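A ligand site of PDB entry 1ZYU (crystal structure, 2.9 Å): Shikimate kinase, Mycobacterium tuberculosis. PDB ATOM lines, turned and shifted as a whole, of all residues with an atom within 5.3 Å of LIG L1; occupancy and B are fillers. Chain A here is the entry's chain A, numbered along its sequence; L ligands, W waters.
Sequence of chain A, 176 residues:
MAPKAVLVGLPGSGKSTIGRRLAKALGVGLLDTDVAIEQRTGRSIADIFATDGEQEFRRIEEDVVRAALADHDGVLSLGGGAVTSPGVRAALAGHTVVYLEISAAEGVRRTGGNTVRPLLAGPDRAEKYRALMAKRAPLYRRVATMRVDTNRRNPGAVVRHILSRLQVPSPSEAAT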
ATOM      1  N   LEU A  10     -11.712   4.532  10.429  1.00  0.00           N
ATOM      2  CA  LEU A  10     -11.601   3.187   9.878  1.00  0.00           C
ATOM      3  C   LEU A  10     -12.702   2.901   8.861  1.00  0.00           C
ATOM      4  O   LEU A  10     -13.831   3.358   9.010  1.00  0.00           O
ATOM      5  CB  LEU A  10     -11.706   2.139  10.987  1.00  0.00           C
ATOM      6  CG  LEU A  10     -10.507   1.906  11.876  1.00  0.00           C
ATOM      7  CD1 LEU A  10     -10.894   0.914  12.970  1.00  0.00           C
ATOM      8  CD2 LEU A  10      -9.339   1.384  11.052  1.00  0.00           C
ATOM      9  N   PRO A  11     -12.379   2.136   7.805  1.00  0.00           N
ATOM     10  CA  PRO A  11     -13.423   1.845   6.817  1.00  0.00           C
ATOM     11  C   PRO A  11     -14.630   1.189   7.506  1.00  0.00           C
ATOM     12  O   PRO A  11     -14.508   0.126   8.118  1.00  0.00           O
ATOM     13  CB  PRO A  11     -12.721   0.921   5.822  1.00  0.00           C
ATOM     14  CG  PRO A  11     -11.607   0.309   6.626  1.00  0.00           C
ATOM     15  CD  PRO A  11     -11.118   1.470   7.445  1.00  0.00           C
ATOM     16  N   GLY A  12     -15.784   1.837   7.394  1.00  0.00           N
ATOM     17  CA  GLY A  12     -16.993   1.338   8.009  1.00  0.00           C
ATOM     18  C   GLY A  12     -17.485   2.257   9.120  1.00  0.00           C
ATOM     19  O   GLY A  12     -18.551   2.017   9.705  1.00  0.00           O
ATOM     20  N   SER A  13     -16.724   3.306   9.411  1.00  0.00           N
ATOM     21  CA  SER A  13     -17.089   4.245  10.456  1.00  0.00           C
ATOM     22  C   SER A  13     -18.126   5.273  10.036  1.00  0.00           C
ATOM     23  O   SER A  13     -18.588   6.059  10.853  1.00  0.00           O
ATOM     24  CB  SER A  13     -15.837   4.955  10.997  1.00  0.00           C
ATOM     25  OG  SER A  13     -15.176   5.692   9.989  1.00  0.00           O
ATOM     26  N   GLY A  14     -18.479   5.285   8.760  1.00  0.00           N
ATOM     27  CA  GLY A  14     -19.479   6.234   8.295  1.00  0.00           C
ATOM     28  C   GLY A  14     -18.974   7.324   7.366  1.00  0.00           C
ATOM     29  O   GLY A  14     -19.774   8.003   6.736  1.00  0.00           O
ATOM     30  N   LYS A  15     -17.654   7.499   7.282  1.00  0.00           N
ATOM     31  CA  LYS A  15     -17.022   8.517   6.441  1.00  0.00           C
ATOM     32  C   LYS A  15     -17.866   9.017   5.261  1.00  0.00           C
ATOM     33  O   LYS A  15     -17.875  10.213   4.959  1.00  0.00           O
ATOM     34  CB  LYS A  15     -15.672   8.018   5.910  1.00  0.00           C
ATOM     35  CG  LYS A  15     -14.493   8.188   6.865  1.00  0.00           C
ATOM     36  CD  LYS A  15     -13.243   7.566   6.266  1.00  0.00           C
ATOM     37  CE  LYS A  15     -13.420   6.056   6.069  1.00  0.00           C
ATOM     38  NZ  LYS A  15     -12.249   5.404   5.404  1.00  0.00           N
ATOM     39  N   SER A  16     -18.551   8.103   4.578  1.00  0.00           N
ATOM     40  CA  SER A  16     -19.371   8.468   3.431  1.00  0.00           C
ATOM     41  C   SER A  16     -20.778   8.897   3.825  1.00  0.00           C
ATOM     42  O   SER A  16     -21.218   9.991   3.469  1.00  0.00           O
ATOM     43  CB  SER A  16     -19.453   7.302   2.441  1.00  0.00           C
ATOM     44  OG  SER A  16     -20.100   6.188   3.031  1.00  0.00           O
ATOM     45  N   THR A  17     -21.496   8.035   4.542  1.00  0.00           N
ATOM     46  CA  THR A  17     -22.850   8.365   4.975  1.00  0.00           C
ATOM     47  C   THR A  17     -22.847   9.756   5.610  1.00  0.00           C
ATOM     48  O   THR A  17     -23.620  10.621   5.226  1.00  0.00           O
ATOM     49  CB  THR A  17     -23.365   7.355   6.032  1.00  0.00           C
ATOM     50  OG1 THR A  17     -23.491   6.053   5.444  1.00  0.00           O
ATOM     51  CG2 THR A  17     -24.707   7.804   6.569  1.00  0.00           C
ATOM     52  N   ILE A  18     -21.956   9.935   6.583  1.00  0.00           N
ATOM     53  CA  ILE A  18     -21.811  11.190   7.312  1.00  0.00           C
ATOM     54  C   ILE A  18     -21.187  12.314   6.492  1.00  0.00           C
ATOM     55  O   ILE A  18     -21.586  13.474   6.616  1.00  0.00           O
ATOM     56  CB  ILE A  18     -20.985  10.942   8.595  1.00  0.00           C
ATOM     57  CG1 ILE A  18     -21.754   9.985   9.504  1.00  0.00           C
ATOM     58  CG2 ILE A  18     -20.696  12.259   9.308  1.00  0.00           C
ATOM     59  CD1 ILE A  18     -21.002   9.563  10.738  1.00  0.00           C
ATOM     60  N   ASP A  32     -14.100  12.631  -1.733  1.00  0.00           N
ATOM     61  CA  ASP A  32     -13.430  11.451  -1.218  1.00  0.00           C
ATOM     62  C   ASP A  32     -12.050  11.275  -1.857  1.00  0.00           C
ATOM     63  O   ASP A  32     -11.904  11.420  -3.059  1.00  0.00           O
ATOM     64  CB  ASP A  32     -14.259  10.190  -1.475  1.00  0.00           C
ATOM     65  CG  ASP A  32     -13.652   8.951  -0.843  1.00  0.00           C
ATOM     66  OD1 ASP A  32     -13.623   8.876   0.404  1.00  0.00           O
ATOM     67  OD2 ASP A  32     -13.203   8.056  -1.585  1.00  0.00           O
ATOM     68  N   ASP A  34     -10.310   8.476  -1.877  1.00  0.00           N
ATOM     69  CA  ASP A  34     -10.245   7.197  -2.572  1.00  0.00           C
ATOM     70  C   ASP A  34     -10.797   7.394  -3.971  1.00  0.00           C
ATOM     71  O   ASP A  34     -10.326   6.767  -4.919  1.00  0.00           O
ATOM     72  CB  ASP A  34     -11.055   6.120  -1.827  1.00  0.00           C
ATOM     73  CG  ASP A  34     -10.451   5.765  -0.481  1.00  0.00           C
ATOM     74  OD1 ASP A  34      -9.208   5.686  -0.383  1.00  0.00           O
ATOM     75  OD2 ASP A  34     -11.231   5.545   0.473  1.00  0.00           O
ATOM     76  N   LEU A  78     -11.076  11.133   4.102  1.00  0.00           N
ATOM     77  CA  LEU A  78      -9.826  10.406   3.857  1.00  0.00           C
ATOM     78  C   LEU A  78      -9.958   8.891   3.921  1.00  0.00           C
ATOM     79  O   LEU A  78     -10.749   8.340   4.691  1.00  0.00           O
ATOM     80  CB  LEU A  78      -8.740  10.846   4.840  1.00  0.00           C
ATOM     81  CG  LEU A  78      -8.254  12.298   4.792  1.00  0.00           C
ATOM     82  CD1 LEU A  78      -6.996  12.418   5.615  1.00  0.00           C
ATOM     83  CD2 LEU A  78      -7.973  12.712   3.367  1.00  0.00           C
ATOM     84  N   GLY A  79      -9.157   8.212   3.102  1.00  0.00           N
ATOM     85  CA  GLY A  79      -9.161   6.761   3.074  1.00  0.00           C
ATOM     86  C   GLY A  79      -8.698   6.238   4.423  1.00  0.00           C
ATOM     87  O   GLY A  79      -8.019   6.937   5.160  1.00  0.00           O
ATOM     88  N   GLY A  80      -9.082   4.998   4.742  1.00  0.00           N
ATOM     89  CA  GLY A  80      -8.689   4.425   6.014  1.00  0.00           C
ATOM     90  C   GLY A  80      -7.245   4.693   6.402  1.00  0.00           C
ATOM     91  O   GLY A  80      -6.974   5.489   7.307  1.00  0.00           O
ATOM     92  N   GLU A 106     -19.459  -2.984  15.437  1.00  0.00           N
ATOM     93  CA  GLU A 106     -20.152  -2.346  14.316  1.00  0.00           C
ATOM     94  C   GLU A 106     -19.294  -2.185  13.073  1.00  0.00           C
ATOM     95  O   GLU A 106     -19.768  -2.408  11.964  1.00  0.00           O
ATOM     96  CB  GLU A 106     -20.707  -0.975  14.735  1.00  0.00           C
ATOM     97  CG  GLU A 106     -22.202  -1.005  15.045  1.00  0.00           C
ATOM     98  CD  GLU A 106     -23.059  -1.366  13.834  1.00  0.00           C
ATOM     99  OE1 GLU A 106     -23.300  -0.483  12.985  1.00  0.00           O
ATOM    100  OE2 GLU A 106     -23.488  -2.534  13.718  1.00  0.00           O
ATOM    101  N   ARG A 110     -20.689  -3.307   9.432  1.00  0.00           N
ATOM    102  CA  ARG A 110     -20.991  -2.329   8.385  1.00  0.00           C
ATOM    103  C   ARG A 110     -20.124  -2.495   7.139  1.00  0.00           C
ATOM    104  O   ARG A 110     -20.279  -1.767   6.161  1.00  0.00           O
ATOM    105  CB  ARG A 110     -20.802  -0.904   8.912  1.00  0.00           C
ATOM    106  CG  ARG A 110     -21.700  -0.525  10.077  1.00  0.00           C
ATOM    107  CD  ARG A 110     -21.341   0.843  10.612  1.00  0.00           C
ATOM    108  NE  ARG A 110     -22.207   1.211  11.734  1.00  0.00           N
ATOM    109  CZ  ARG A 110     -22.036   2.302  12.490  1.00  0.00           C
ATOM    110  NH1 ARG A 110     -21.035   3.133  12.254  1.00  0.00           N
ATOM    111  NH2 ARG A 110     -22.875   2.551  13.485  1.00  0.00           N
ATOM    112  N   ARG A 117     -12.460  -4.468  -0.727  1.00  0.00           N
ATOM    113  CA  ARG A 117     -11.575  -3.838   0.246  1.00  0.00           C
ATOM    114  C   ARG A 117     -10.264  -4.619   0.362  1.00  0.00           C
ATOM    115  O   ARG A 117     -10.205  -5.668   1.007  1.00  0.00           O
ATOM    116  CB  ARG A 117     -12.219  -3.769   1.631  1.00  0.00           C
ATOM    117  CG  ARG A 117     -13.534  -3.028   1.679  1.00  0.00           C
ATOM    118  CD  ARG A 117     -14.214  -3.192   3.027  1.00  0.00           C
ATOM    119  NE  ARG A 117     -15.590  -2.722   2.959  1.00  0.00           N
ATOM    120  CZ  ARG A 117     -15.916  -1.465   2.705  1.00  0.00           C
ATOM    121  NH1 ARG A 117     -14.972  -0.549   2.512  1.00  0.00           N
ATOM    122  NH2 ARG A 117     -17.205  -1.120   2.617  1.00  0.00           N
ATOM    123  N   THR A 150     -19.557   7.322  16.164  1.00  0.00           N
ATOM    124  CA  THR A 150     -20.644   7.008  15.227  1.00  0.00           C
ATOM    125  C   THR A 150     -21.123   5.592  15.466  1.00  0.00           C
ATOM    126  O   THR A 150     -21.855   5.036  14.664  1.00  0.00           O
ATOM    127  CB  THR A 150     -20.184   7.072  13.752  1.00  0.00           C
ATOM    128  OG1 THR A 150     -19.373   5.940  13.458  1.00  0.00           O
ATOM    129  CG2 THR A 150     -19.397   8.348  13.475  1.00  0.00           C
ATOM    130  N   ASN A 151     -20.691   5.020  16.589  1.00  0.00           N
ATOM    131  CA  ASN A 151     -21.070   3.652  16.916  1.00  0.00           C
ATOM    132  C   ASN A 151     -22.573   3.557  17.075  1.00  0.00           C
ATOM    133  O   ASN A 151     -23.311   3.450  16.082  1.00  0.00           O
ATOM    134  CB  ASN A 151     -20.395   3.209  18.214  1.00  0.00           C
ATOM    135  CG  ASN A 151     -19.776   1.828  18.106  1.00  0.00           C
ATOM    136  OD1 ASN A 151     -20.411   0.892  17.619  1.00  0.00           O
ATOM    137  ND2 ASN A 151     -18.538   1.689  18.566  1.00  0.00           N
ATOM    138  N   ARG A 153     -25.557   5.059  17.029  1.00  0.00           N
ATOM    139  CA  ARG A 153     -26.083   6.344  16.622  1.00  0.00           C
ATOM    140  C   ARG A 153     -26.804   6.257  15.277  1.00  0.00           C
ATOM    141  O   ARG A 153     -26.659   5.278  14.542  1.00  0.00           O
ATOM    142  CB  ARG A 153     -24.950   7.378  16.537  1.00  0.00           C
ATOM    143  CG  ARG A 153     -25.303   8.744  17.105  1.00  0.00           C
ATOM    144  CD  ARG A 153     -24.319   9.176  18.188  1.00  0.00           C
ATOM    145  NE  ARG A 153     -24.632  10.496  18.735  1.00  0.00           N
ATOM    146  CZ  ARG A 153     -23.907  11.139  19.644  1.00  0.00           C
ATOM    147  NH1 ARG A 153     -22.791  10.594  20.123  1.00  0.00           N
ATOM    148  NH2 ARG A 153     -24.280  12.335  20.076  1.00  0.00           N
ATOM    149  N   ASN A 154     -27.612   7.275  14.998  1.00  0.00           N
ATOM    150  CA  ASN A 154     -28.362   7.373  13.757  1.00  0.00           C
ATOM    151  C   ASN A 154     -27.494   8.233  12.832  1.00  0.00           C
ATOM    152  O   ASN A 154     -27.102   9.337  13.209  1.00  0.00           O
ATOM    153  CB  ASN A 154     -29.728   8.028  14.024  1.00  0.00           C
ATOM    154  CG  ASN A 154     -30.351   8.634  12.782  1.00  0.00           C
ATOM    155  OD1 ASN A 154     -30.057   8.222  11.657  1.00  0.00           O
ATOM    156  ND2 ASN A 154     -31.238   9.605  12.978  1.00  0.00           N
ATOM    157  N   PRO A 155     -27.173   7.736  11.630  1.00  0.00           N
ATOM    158  CA  PRO A 155     -26.359   8.479  10.672  1.00  0.00           C
ATOM    159  C   PRO A 155     -26.594   9.989  10.679  1.00  0.00           C
ATOM    160  O   PRO A 155     -25.662  10.775  10.457  1.00  0.00           O
ATOM    161  CB  PRO A 155     -26.713   7.826   9.349  1.00  0.00           C
ATOM    162  CG  PRO A 155     -26.822   6.392   9.744  1.00  0.00           C
ATOM    163  CD  PRO A 155     -27.632   6.462  11.045  1.00  0.00           C
ATOM    164  N   VAL A 158     -25.613  11.883  14.216  1.00  0.00           N
ATOM    165  CA  VAL A 158     -24.175  12.049  14.333  1.00  0.00           C
ATOM    166  C   VAL A 158     -23.815  13.394  13.719  1.00  0.00           C
ATOM    167  O   VAL A 158     -23.015  14.143  14.278  1.00  0.00           O
ATOM    168  CB  VAL A 158     -23.427  10.943  13.591  1.00  0.00           C
ATOM    169  CG1 VAL A 158     -21.928  11.159  13.714  1.00  0.00           C
ATOM    170  CG2 VAL A 158     -23.837   9.590  14.152  1.00  0.00           C
HETATM  171  P1  LIG L   1     -14.703   3.286   3.121  1.00  0.00           P
HETATM  172  O1  LIG L   1     -13.598   4.026   3.802  1.00  0.00           O
HETATM  173  O2  LIG L   1     -14.342   1.952   2.630  1.00  0.00           O
HETATM  174  O3  LIG L   1     -15.203   4.120   1.978  1.00  0.00           O
HETATM  175  P2  LIG L   1     -16.784   4.034   5.084  1.00  0.00           P
HETATM  176  O4  LIG L   1     -16.222   4.383   6.391  1.00  0.00           O
HETATM  177  O5  LIG L   1     -17.078   5.183   4.151  1.00  0.00           O
HETATM  178  C1  LIG L   1     -15.812   2.983   4.294  1.00  0.00           C
HETATM  179  P3  LIG L   1     -19.764   3.919   5.149  1.00  0.00           P
HETATM  180  O6  LIG L   1     -20.092   3.500   3.817  1.00  0.00           O
HETATM  181  O7  LIG L   1     -19.947   5.238   5.500  1.00  0.00           O
HETATM  182  O8  LIG L   1     -18.159   3.342   5.423  1.00  0.00           O
HETATM  183  O9  LIG L   1     -20.847   3.029   6.085  1.00  0.00           O
HETATM  184  C2  LIG L   1     -20.918   1.599   5.975  1.00  0.00           C
HETATM  185  C3  LIG L   1     -22.281   1.167   6.480  1.00  0.00           C
HETATM  186  O10 LIG L   1     -22.345   1.846   7.882  1.00  0.00           O
HETATM  187  C4  LIG L   1     -23.567   1.697   5.782  1.00  0.00           C
HETATM  188  O11 LIG L   1     -24.340   0.547   5.722  1.00  0.00           O
HETATM  189  C5  LIG L   1     -24.112   2.806   6.700  1.00  0.00           C
HETATM  190  O12 LIG L   1     -25.563   2.757   6.580  1.00  0.00           O
HETATM  191  C6  LIG L   1     -23.617   2.452   8.080  1.00  0.00           C
HETATM  192  N1  LIG L   1     -23.442   3.646   8.980  1.00  0.00           N
HETATM  193  C7  LIG L   1     -22.665   4.756   8.702  1.00  0.00           C
HETATM  194  N2  LIG L   1     -22.693   5.677   9.597  1.00  0.00           N
HETATM  195  C8  LIG L   1     -23.491   5.143  10.583  1.00  0.00           C
HETATM  196  C9  LIG L   1     -23.936   5.668  11.867  1.00  0.00           C
HETATM  197  N3  LIG L   1     -23.585   6.864  12.288  1.00  0.00           N
HETATM  198  N4  LIG L   1     -24.916   4.958  12.621  1.00  0.00           N
HETATM  199  C10 LIG L   1     -25.450   3.787  12.122  1.00  0.00           C
HETATM  200  N5  LIG L   1     -24.985   3.124  10.982  1.00  0.00           N
HETATM  201  C11 LIG L   1     -24.090   3.950  10.195  1.00  0.00           C
HETATM  202  O1  LG2 L   2      -8.449   3.286   0.514  1.00  0.00           O
HETATM  203  C1  LG2 L   2      -9.164   2.055   0.476  1.00  0.00           C
HETATM  204  C2  LG2 L   2      -8.167   0.880   0.472  1.00  0.00           C
HETATM  205  O2  LG2 L   2      -8.893  -0.350   0.412  1.00  0.00           O
HETATM  206  C3  LG2 L   2      -7.298   0.866   1.760  1.00  0.00           C
HETATM  207  C4  LG2 L   2      -8.077   1.217   3.043  1.00  0.00           C
HETATM  208  C5  LG2 L   2      -7.411   0.987   4.352  1.00  0.00           C
HETATM  209  O3  LG2 L   2      -7.999   0.479   5.310  1.00  0.00           O
HETATM  210  O4  LG2 L   2      -6.121   1.341   4.560  1.00  0.00           O
HETATM  211  C6  LG2 L   2      -9.343   1.737   3.005  1.00  0.00           C
HETATM  212  C7  LG2 L   2     -10.093   2.002   1.719  1.00  0.00           C
HETATM  213  O5  LG2 L   2     -10.777   3.255   1.822  1.00  0.00           O
HETATM  214  O   HOH W   1     -12.969   0.509  -0.190  1.00  0.00           O
HETATM  215  O   HOH W   2     -15.862   7.319   2.700  1.00  0.00           O
HETATM  216  O   HOH W   3     -23.316  -1.762   6.191  1.00  0.00           O
HETATM  217  O   HOH W   4     -17.864   1.481   2.965  1.00  0.00           O
HETATM  218  O   HOH W   5     -16.542   2.351   0.040  1.00  0.00           O
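The backbone carbonyl oxygen (O) of Ser 13 is in hydrogen-bond range of the side-chain hydroxyl (OG1) of Thr 150, 2.7 Å away. The side-chain hydroxyl (OG) of Ser 13 sits at hydrogen-bond distance from the backbone carbonyl oxygen (O) of Leu 10, 2.9 Å away. The side-chain carboxylate of Glu 106 lies within salt-bridge range of the guanidinium group of Arg 110 (3.1 Å). The guanidinium group of Arg 110 sits at hydrogen-bond distance from the backbone carbonyl oxygen of Asn 151, 2.8 Å away. The backbone carbonyl oxygen of Leu 78 sits close to the side-chain amino group of Lys 15 (3.4 Å). O of Thr 150 lies within hydrogen-bond range of NH2 of Arg 110, 2.9 Å away.
The backbone carbonyl oxygen (O) of Gly 14 sits close to an oxygen (O7) of LIG L1, at 3.0 Å. The backbone carbonyl oxygen of Thr 150 sits at hydrogen-bond distance from a nitrogen (N3) of LIG L1 (3.5 Å). The side-chain carboxylate (OD1) of Asp 34 is in hydrogen-bond range of an oxygen (O1) of LG2 L2 (2.7 Å). NZ of Lys 15 is in salt-bridge range of O1 of LIG L1 (2.5 Å). O7 of LIG L1 lies within hydrogen-bond range of OG of Ser 16 (2.6 Å). The guanidinium group of Arg 117 lies within salt-bridge range of an oxygen (O2) of LIG L1 (2.6 Å). The backbone NH of Gly 12 sits at hydrogen-bond distance from an oxygen (O4) of LIG L1 (2.8 Å). The guanidinium group (NH2) of Arg 110 lies close to a nitrogen (N4) of LIG L1 (3.3 Å). The backbone NH of Thr 17 lies within hydrogen-bond range of an oxygen (O7) of LIG L1, at 3.3 Å. O of Arg 153 sits close to N4 of LIG L1 (2.6 Å). The backbone NH of Ser 16 lies within hydrogen-bond range of an oxygen (O5) of LIG L1, at 3.3 Å. An oxygen (O4) of LIG L1 is in hydrogen-bond range of the backbone NH (N) of Gly 14, 3.4 Å away. N of Ser 13 is in hydrogen-bond range of O4 of LIG L1 (3.2 Å).
Merely in contact with LIG L1: Leu 10 (3.7 Å), Pro 11 (3.7 Å), Pro 155 (3.5 Å) and Val 158 (3.3 Å). Of the 23 residues printed, 14 come within 4 Å of LIG L1. The nearest printed residue that does not touch LIG L1 is Ile 18 (4.04 Å).
Water W3 lies within hydrogen-bond range of an oxygen (O11) of LIG L1 (2.6 Å) and the backbone carbonyl oxygen of Arg 110 (3.0 Å). Water W2 bridges an oxygen (O5) of LIG L1 (2.9 Å) and the backbone NH of Ser 16 (3.4 Å). Water W4 bridges NH2 of Arg 117 and O8 of LIG L1.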
